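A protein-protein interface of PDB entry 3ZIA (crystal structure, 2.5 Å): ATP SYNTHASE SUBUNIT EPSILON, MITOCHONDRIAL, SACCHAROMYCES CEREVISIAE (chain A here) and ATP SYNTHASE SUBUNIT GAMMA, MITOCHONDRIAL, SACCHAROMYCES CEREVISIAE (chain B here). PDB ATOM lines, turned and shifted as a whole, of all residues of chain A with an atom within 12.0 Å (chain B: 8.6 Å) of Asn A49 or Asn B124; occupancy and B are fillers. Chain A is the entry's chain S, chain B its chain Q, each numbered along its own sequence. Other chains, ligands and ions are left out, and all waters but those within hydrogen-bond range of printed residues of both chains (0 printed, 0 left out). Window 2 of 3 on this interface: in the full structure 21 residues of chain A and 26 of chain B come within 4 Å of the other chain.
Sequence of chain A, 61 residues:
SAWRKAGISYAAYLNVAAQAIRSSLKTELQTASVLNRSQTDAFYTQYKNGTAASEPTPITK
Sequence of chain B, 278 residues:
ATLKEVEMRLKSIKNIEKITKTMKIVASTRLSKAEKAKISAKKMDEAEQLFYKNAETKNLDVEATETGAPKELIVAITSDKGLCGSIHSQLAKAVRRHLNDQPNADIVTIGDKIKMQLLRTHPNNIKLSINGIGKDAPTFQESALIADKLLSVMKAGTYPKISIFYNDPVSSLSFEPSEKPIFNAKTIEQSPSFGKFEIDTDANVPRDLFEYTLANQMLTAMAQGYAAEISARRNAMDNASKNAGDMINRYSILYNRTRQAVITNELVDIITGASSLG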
ATOM      1  N   THR A  45       5.462 -36.409 -29.605  1.00  0.00           N
ATOM      2  CA  THR A  45       5.550 -35.429 -28.529  1.00  0.00           C
ATOM      3  C   THR A  45       4.179 -35.201 -27.899  1.00  0.00           C
ATOM      4  O   THR A  45       3.214 -34.874 -28.593  1.00  0.00           O
ATOM      5  CB  THR A  45       6.115 -34.082 -29.035  1.00  0.00           C
ATOM      6  OG1 THR A  45       7.172 -34.316 -29.976  1.00  0.00           O
ATOM      7  CG2 THR A  45       6.646 -33.252 -27.875  1.00  0.00           C
ATOM      8  N   GLN A  46       4.103 -35.379 -26.584  1.00  0.00           N
ATOM      9  CA  GLN A  46       2.855 -35.182 -25.848  1.00  0.00           C
ATOM     10  C   GLN A  46       2.655 -33.692 -25.566  1.00  0.00           C
ATOM     11  O   GLN A  46       3.624 -32.969 -25.368  1.00  0.00           O
ATOM     12  CB  GLN A  46       2.871 -35.993 -24.546  1.00  0.00           C
ATOM     13  CG  GLN A  46       1.486 -36.410 -24.048  1.00  0.00           C
ATOM     14  CD  GLN A  46       1.531 -37.419 -22.909  1.00  0.00           C
ATOM     15  OE1 GLN A  46       2.557 -38.050 -22.655  1.00  0.00           O
ATOM     16  NE2 GLN A  46       0.406 -37.580 -22.222  1.00  0.00           N
ATOM     17  N   TYR A  47       1.400 -33.242 -25.565  1.00  0.00           N
ATOM     18  CA  TYR A  47       1.069 -31.828 -25.340  1.00  0.00           C
ATOM     19  C   TYR A  47       0.027 -31.615 -24.239  1.00  0.00           C
ATOM     20  O   TYR A  47      -0.935 -32.381 -24.112  1.00  0.00           O
ATOM     21  CB  TYR A  47       0.571 -31.186 -26.635  1.00  0.00           C
ATOM     22  CG  TYR A  47       1.657 -30.650 -27.543  1.00  0.00           C
ATOM     23  CD1 TYR A  47       2.427 -31.510 -28.334  1.00  0.00           C
ATOM     24  CD2 TYR A  47       1.898 -29.279 -27.634  1.00  0.00           C
ATOM     25  CE1 TYR A  47       3.422 -31.015 -29.179  1.00  0.00           C
ATOM     26  CE2 TYR A  47       2.887 -28.774 -28.474  1.00  0.00           C
ATOM     27  CZ  TYR A  47       3.644 -29.647 -29.243  1.00  0.00           C
ATOM     28  OH  TYR A  47       4.618 -29.151 -30.074  1.00  0.00           O
ATOM     29  N   LYS A  48       0.232 -30.564 -23.450  1.00  0.00           N
ATOM     30  CA  LYS A  48      -0.711 -30.172 -22.404  1.00  0.00           C
ATOM     31  C   LYS A  48      -0.950 -28.667 -22.419  1.00  0.00           C
ATOM     32  O   LYS A  48      -0.091 -27.901 -22.867  1.00  0.00           O
ATOM     33  CB  LYS A  48      -0.219 -30.610 -21.019  1.00  0.00           C
ATOM     34  CG  LYS A  48      -0.463 -32.084 -20.694  1.00  0.00           C
ATOM     35  CD  LYS A  48      -0.831 -32.278 -19.224  1.00  0.00           C
ATOM     36  CE  LYS A  48      -2.320 -32.033 -18.992  1.00  0.00           C
ATOM     37  NZ  LYS A  48      -2.626 -31.757 -17.567  1.00  0.00           N
ATOM     38  N   ASN A  49      -2.121 -28.260 -21.927  1.00  0.00           N
ATOM     39  CA  ASN A  49      -2.524 -26.845 -21.834  1.00  0.00           C
ATOM     40  C   ASN A  49      -2.570 -26.121 -23.179  1.00  0.00           C
ATOM     41  O   ASN A  49      -2.508 -26.747 -24.240  1.00  0.00           O
ATOM     42  CB  ASN A  49      -1.639 -26.075 -20.838  1.00  0.00           C
ATOM     43  CG  ASN A  49      -1.797 -26.571 -19.413  1.00  0.00           C
ATOM     44  OD1 ASN A  49      -2.710 -26.155 -18.698  1.00  0.00           O
ATOM     45  ND2 ASN A  49      -0.901 -27.462 -18.991  1.00  0.00           N
ATOM     46  N   ALA A  53      -0.098 -24.593 -24.429  1.00  0.00           N
ATOM     47  CA  ALA A  53       0.267 -25.413 -25.580  1.00  0.00           C
ATOM     48  C   ALA A  53       1.742 -25.825 -25.546  1.00  0.00           C
ATOM     49  O   ALA A  53       2.390 -25.966 -26.590  1.00  0.00           O
ATOM     50  CB  ALA A  53      -0.069 -24.685 -26.875  1.00  0.00           C
ATOM     51  N   SER A  54       2.262 -26.013 -24.336  1.00  0.00           N
ATOM     52  CA  SER A  54       3.604 -26.546 -24.143  1.00  0.00           C
ATOM     53  C   SER A  54       3.569 -28.077 -24.202  1.00  0.00           C
ATOM     54  O   SER A  54       2.541 -28.672 -24.542  1.00  0.00           O
ATOM     55  CB  SER A  54       4.201 -26.060 -22.818  1.00  0.00           C
ATOM     56  OG  SER A  54       3.687 -26.790 -21.716  1.00  0.00           O
ATOM     57  N   GLU A  55       4.690 -28.705 -23.855  1.00  0.00           N
ATOM     58  CA  GLU A  55       4.869 -30.140 -24.043  1.00  0.00           C
ATOM     59  C   GLU A  55       6.102 -30.664 -23.297  1.00  0.00           C
ATOM     60  O   GLU A  55       7.072 -29.924 -23.116  1.00  0.00           O
ATOM     61  CB  GLU A  55       4.968 -30.462 -25.546  1.00  0.00           C
ATOM     62  CG  GLU A  55       6.223 -29.946 -26.281  1.00  0.00           C
ATOM     63  CD  GLU A  55       6.273 -28.434 -26.429  1.00  0.00           C
ATOM     64  OE1 GLU A  55       6.408 -27.732 -25.406  1.00  0.00           O
ATOM     65  OE2 GLU A  55       6.205 -27.944 -27.576  1.00  0.00           O
ATOM     66  N   PRO A  56       6.058 -31.933 -22.843  1.00  0.00           N
ATOM     67  CA  PRO A  56       7.245 -32.609 -22.308  1.00  0.00           C
ATOM     68  C   PRO A  56       8.060 -33.350 -23.374  1.00  0.00           C
ATOM     69  O   PRO A  56       7.494 -33.870 -24.336  1.00  0.00           O
ATOM     70  CB  PRO A  56       6.664 -33.622 -21.308  1.00  0.00           C
ATOM     71  CG  PRO A  56       5.176 -33.410 -21.303  1.00  0.00           C
ATOM     72  CD  PRO A  56       4.834 -32.701 -22.561  1.00  0.00           C
ATOM     73  N   PRO B 103     -16.589 -29.249 -29.425  1.00  0.00           N
ATOM     74  CA  PRO B 103     -15.408 -28.438 -29.094  1.00  0.00           C
ATOM     75  C   PRO B 103     -14.492 -28.996 -27.996  1.00  0.00           C
ATOM     76  O   PRO B 103     -13.422 -28.428 -27.747  1.00  0.00           O
ATOM     77  CB  PRO B 103     -16.026 -27.110 -28.642  1.00  0.00           C
ATOM     78  CG  PRO B 103     -17.363 -27.492 -28.059  1.00  0.00           C
ATOM     79  CD  PRO B 103     -17.783 -28.814 -28.674  1.00  0.00           C
ATOM     80  N   ASN B 104     -14.900 -30.088 -27.352  1.00  0.00           N
ATOM     81  CA  ASN B 104     -14.143 -30.642 -26.225  1.00  0.00           C
ATOM     82  C   ASN B 104     -13.284 -31.861 -26.588  1.00  0.00           C
ATOM     83  O   ASN B 104     -12.609 -32.426 -25.720  1.00  0.00           O
ATOM     84  CB  ASN B 104     -15.085 -30.976 -25.061  1.00  0.00           C
ATOM     85  CG  ASN B 104     -16.006 -32.142 -25.374  1.00  0.00           C
ATOM     86  OD1 ASN B 104     -16.706 -32.149 -26.393  1.00  0.00           O
ATOM     87  ND2 ASN B 104     -16.005 -33.143 -24.499  1.00  0.00           N
ATOM     88  N   ALA B 105     -13.315 -32.248 -27.869  1.00  0.00           N
ATOM     89  CA  ALA B 105     -12.575 -33.411 -28.385  1.00  0.00           C
ATOM     90  C   ALA B 105     -11.055 -33.273 -28.265  1.00  0.00           C
ATOM     91  O   ALA B 105     -10.507 -32.165 -28.328  1.00  0.00           O
ATOM     92  CB  ALA B 105     -12.967 -33.687 -29.837  1.00  0.00           C
ATOM     93  N   ASP B 106     -10.384 -34.409 -28.086  1.00  0.00           N
ATOM     94  CA  ASP B 106      -8.922 -34.455 -28.086  1.00  0.00           C
ATOM     95  C   ASP B 106      -8.375 -34.618 -29.508  1.00  0.00           C
ATOM     96  O   ASP B 106      -8.974 -35.300 -30.356  1.00  0.00           O
ATOM     97  CB  ASP B 106      -8.403 -35.575 -27.175  1.00  0.00           C
ATOM     98  CG  ASP B 106      -8.567 -35.260 -25.688  1.00  0.00           C
ATOM     99  OD1 ASP B 106      -8.904 -34.106 -25.330  1.00  0.00           O
ATOM    100  OD2 ASP B 106      -8.349 -36.184 -24.871  1.00  0.00           O
ATOM    101  N   ILE B 107      -7.237 -33.978 -29.761  1.00  0.00           N
ATOM    102  CA  ILE B 107      -6.621 -34.003 -31.081  1.00  0.00           C
ATOM    103  C   ILE B 107      -5.225 -34.611 -31.036  1.00  0.00           C
ATOM    104  O   ILE B 107      -4.398 -34.241 -30.196  1.00  0.00           O
ATOM    105  CB  ILE B 107      -6.541 -32.582 -31.711  1.00  0.00           C
ATOM    106  CG1 ILE B 107      -7.908 -31.891 -31.664  1.00  0.00           C
ATOM    107  CG2 ILE B 107      -6.021 -32.655 -33.153  1.00  0.00           C
ATOM    108  CD1 ILE B 107      -7.868 -30.421 -32.006  1.00  0.00           C
ATOM    109  N   LEU B 118      -3.787 -25.973 -36.165  1.00  0.00           N
ATOM    110  CA  LEU B 118      -4.666 -26.264 -35.035  1.00  0.00           C
ATOM    111  C   LEU B 118      -4.120 -25.723 -33.716  1.00  0.00           C
ATOM    112  O   LEU B 118      -4.861 -25.572 -32.750  1.00  0.00           O
ATOM    113  CB  LEU B 118      -4.919 -27.770 -34.948  1.00  0.00           C
ATOM    114  CG  LEU B 118      -5.978 -28.405 -35.867  1.00  0.00           C
ATOM    115  CD1 LEU B 118      -6.162 -27.718 -37.220  1.00  0.00           C
ATOM    116  CD2 LEU B 118      -5.667 -29.877 -36.074  1.00  0.00           C
ATOM    117  N   LEU B 119      -2.826 -25.414 -33.691  1.00  0.00           N
ATOM    118  CA  LEU B 119      -2.185 -24.832 -32.512  1.00  0.00           C
ATOM    119  C   LEU B 119      -2.513 -23.346 -32.362  1.00  0.00           C
ATOM    120  O   LEU B 119      -2.455 -22.796 -31.261  1.00  0.00           O
ATOM    121  CB  LEU B 119      -0.670 -25.037 -32.575  1.00  0.00           C
ATOM    122  CG  LEU B 119       0.094 -25.184 -31.257  1.00  0.00           C
ATOM    123  CD1 LEU B 119      -0.650 -26.079 -30.277  1.00  0.00           C
ATOM    124  CD2 LEU B 119       1.485 -25.735 -31.523  1.00  0.00           C
ATOM    125  N   ARG B 120      -2.851 -22.708 -33.481  1.00  0.00           N
ATOM    126  CA  ARG B 120      -3.271 -21.309 -33.498  1.00  0.00           C
ATOM    127  C   ARG B 120      -4.728 -21.199 -33.030  1.00  0.00           C
ATOM    128  O   ARG B 120      -5.034 -20.497 -32.061  1.00  0.00           O
ATOM    129  CB  ARG B 120      -3.119 -20.733 -34.913  1.00  0.00           C
ATOM    130  CG  ARG B 120      -2.728 -19.265 -34.959  1.00  0.00           C
ATOM    131  CD  ARG B 120      -2.403 -18.835 -36.377  1.00  0.00           C
ATOM    132  NE  ARG B 120      -3.607 -18.565 -37.165  1.00  0.00           N
ATOM    133  CZ  ARG B 120      -4.017 -17.350 -37.526  1.00  0.00           C
ATOM    134  NH1 ARG B 120      -3.323 -16.269 -37.180  1.00  0.00           N
ATOM    135  NH2 ARG B 120      -5.125 -17.212 -38.243  1.00  0.00           N
ATOM    136  N   THR B 121      -5.606 -21.925 -33.720  1.00  0.00           N
ATOM    137  CA  THR B 121      -7.048 -21.867 -33.494  1.00  0.00           C
ATOM    138  C   THR B 121      -7.528 -22.609 -32.228  1.00  0.00           C
ATOM    139  O   THR B 121      -8.234 -22.021 -31.405  1.00  0.00           O
ATOM    140  CB  THR B 121      -7.830 -22.324 -34.760  1.00  0.00           C
ATOM    141  OG1 THR B 121      -9.228 -22.404 -34.471  1.00  0.00           O
ATOM    142  CG2 THR B 121      -7.351 -23.673 -35.236  1.00  0.00           C
ATOM    143  N   HIS B 122      -7.138 -23.876 -32.061  1.00  0.00           N
ATOM    144  CA  HIS B 122      -7.577 -24.685 -30.911  1.00  0.00           C
ATOM    145  C   HIS B 122      -6.411 -25.243 -30.078  1.00  0.00           C
ATOM    146  O   HIS B 122      -6.288 -26.463 -29.936  1.00  0.00           O
ATOM    147  CB  HIS B 122      -8.452 -25.847 -31.384  1.00  0.00           C
ATOM    148  CG  HIS B 122      -9.755 -25.423 -31.986  1.00  0.00           C
ATOM    149  ND1 HIS B 122      -9.916 -25.208 -33.338  1.00  0.00           N
ATOM    150  CD2 HIS B 122     -10.964 -25.191 -31.422  1.00  0.00           C
ATOM    151  CE1 HIS B 122     -11.166 -24.856 -33.580  1.00  0.00           C
ATOM    152  NE2 HIS B 122     -11.822 -24.837 -32.434  1.00  0.00           N
ATOM    153  N   PRO B 123      -5.573 -24.357 -29.499  1.00  0.00           N
ATOM    154  CA  PRO B 123      -4.310 -24.802 -28.885  1.00  0.00           C
ATOM    155  C   PRO B 123      -4.441 -25.848 -27.769  1.00  0.00           C
ATOM    156  O   PRO B 123      -3.627 -26.773 -27.700  1.00  0.00           O
ATOM    157  CB  PRO B 123      -3.697 -23.503 -28.338  1.00  0.00           C
ATOM    158  CG  PRO B 123      -4.831 -22.545 -28.229  1.00  0.00           C
ATOM    159  CD  PRO B 123      -5.784 -22.906 -29.323  1.00  0.00           C
ATOM    160  N   ASN B 124      -5.448 -25.711 -26.913  1.00  0.00           N
ATOM    161  CA  ASN B 124      -5.568 -26.583 -25.744  1.00  0.00           C
ATOM    162  C   ASN B 124      -6.073 -27.991 -26.049  1.00  0.00           C
ATOM    163  O   ASN B 124      -5.880 -28.906 -25.248  1.00  0.00           O
ATOM    164  CB  ASN B 124      -6.406 -25.914 -24.647  1.00  0.00           C
ATOM    165  CG  ASN B 124      -5.682 -24.740 -23.995  1.00  0.00           C
ATOM    166  OD1 ASN B 124      -5.160 -23.853 -24.678  1.00  0.00           O
ATOM    167  ND2 ASN B 124      -5.649 -24.730 -22.667  1.00  0.00           N
ATOM    168  N   ASN B 125      -6.702 -28.154 -27.211  1.00  0.00           N
ATOM    169  CA  ASN B 125      -7.272 -29.436 -27.639  1.00  0.00           C
ATOM    170  C   ASN B 125      -6.227 -30.491 -28.012  1.00  0.00           C
ATOM    171  O   ASN B 125      -6.486 -31.697 -27.914  1.00  0.00           O
ATOM    172  CB  ASN B 125      -8.202 -29.222 -28.835  1.00  0.00           C
ATOM    173  CG  ASN B 125      -9.496 -28.512 -28.468  1.00  0.00           C
ATOM    174  OD1 ASN B 125     -10.569 -28.876 -28.959  1.00  0.00           O
ATOM    175  ND2 ASN B 125      -9.405 -27.488 -27.619  1.00  0.00           N
ATOM    176  N   ILE B 126      -5.059 -30.032 -28.452  1.00  0.00           N
ATOM    177  CA  ILE B 126      -3.999 -30.920 -28.924  1.00  0.00           C
ATOM    178  C   ILE B 126      -3.318 -31.595 -27.741  1.00  0.00           C
ATOM    179  O   ILE B 126      -2.821 -30.920 -26.833  1.00  0.00           O
ATOM    180  CB  ILE B 126      -2.964 -30.153 -29.789  1.00  0.00           C
ATOM    181  CG1 ILE B 126      -3.600 -29.709 -31.111  1.00  0.00           C
ATOM    182  CG2 ILE B 126      -1.722 -31.012 -30.054  1.00  0.00           C
ATOM    183  CD1 ILE B 126      -2.877 -28.570 -31.803  1.00  0.00           C
ATOM    184  N   LYS B 127      -3.301 -32.924 -27.750  1.00  0.00           N
ATOM    185  CA  LYS B 127      -2.681 -33.667 -26.658  1.00  0.00           C
ATOM    186  C   LYS B 127      -1.474 -34.507 -27.099  1.00  0.00           C
ATOM    187  O   LYS B 127      -0.683 -34.946 -26.259  1.00  0.00           O
ATOM    188  CB  LYS B 127      -3.719 -34.521 -25.923  1.00  0.00           C
ATOM    189  CG  LYS B 127      -3.408 -34.707 -24.442  1.00  0.00           C
ATOM    190  CD  LYS B 127      -4.302 -35.757 -23.794  1.00  0.00           C
ATOM    191  CE  LYS B 127      -3.668 -36.322 -22.527  1.00  0.00           C
ATOM    192  NZ  LYS B 127      -4.398 -37.523 -22.035  1.00  0.00           N
ATOM    193  N   LEU B 128      -1.326 -34.714 -28.408  1.00  0.00           N
ATOM    194  CA  LEU B 128      -0.207 -35.490 -28.957  1.00  0.00           C
ATOM    195  C   LEU B 128       0.109 -35.139 -30.415  1.00  0.00           C
ATOM    196  O   LEU B 128      -0.780 -35.140 -31.269  1.00  0.00           O
ATOM    197  CB  LEU B 128      -0.483 -36.996 -28.831  1.00  0.00           C
ATOM    198  CG  LEU B 128       0.623 -37.979 -29.220  1.00  0.00           C
ATOM    199  CD1 LEU B 128       1.759 -37.956 -28.207  1.00  0.00           C
ATOM    200  CD2 LEU B 128       0.051 -39.378 -29.343  1.00  0.00           C
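O of Lys B127 sits at hydrogen-bond distance from N of Tyr A47, 2.8 Å away.
Of the 16 printed residues of chain B, 6 touch a printed residue of chain A. Printed residues of chain B that touch a printed residue of chain A: Leu B119, Pro B123, Asn B124, Ile B126, Lys B127 and Leu B128. Hydrophobic or aromatic side chains of chain A within 4 Å of the printed part of chain B: Tyr A47 and Ala A53.
Of chain B, only Pro B123 and Asn B124 come within 4 Å of Asn A49. Of chain A, only Asn A49 comes within 4 Å of Asn B124. Of chain A, only Asn A49 comes within 4 Å of Pro B123. Of the printed residues of chain A, Leu B128 touches Thr A45 (3.4 Å) and Gln A46 (3.8 Å). Of the printed residues of chain B, Thr A45 touches Leu B128 (3.4 Å). Lys A48 touches none of the printed residues of chain B. The nearest residue of chain A that does not touch Asn B124 is Ala A53 (5.1 Å).
Leu B128 touches Thr A45. Gln A46 touches Lys B127. Leu B128 touches Gln A46. O of Ile B126 touches CB of Tyr A47, at 3.4 Å. Asn A49 touches Pro B123 (O to O, 3.6 Å). Asn B124 touches Asn A49. Ala A53 touches Leu B119 (CB to CD1, 3.7 Å).
O of Ile B107 sits at hydrogen-bond distance from N of Lys B127. OH of Tyr A47 lies within hydrogen-bond range of OE2 of Glu A55 (3.2 Å).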
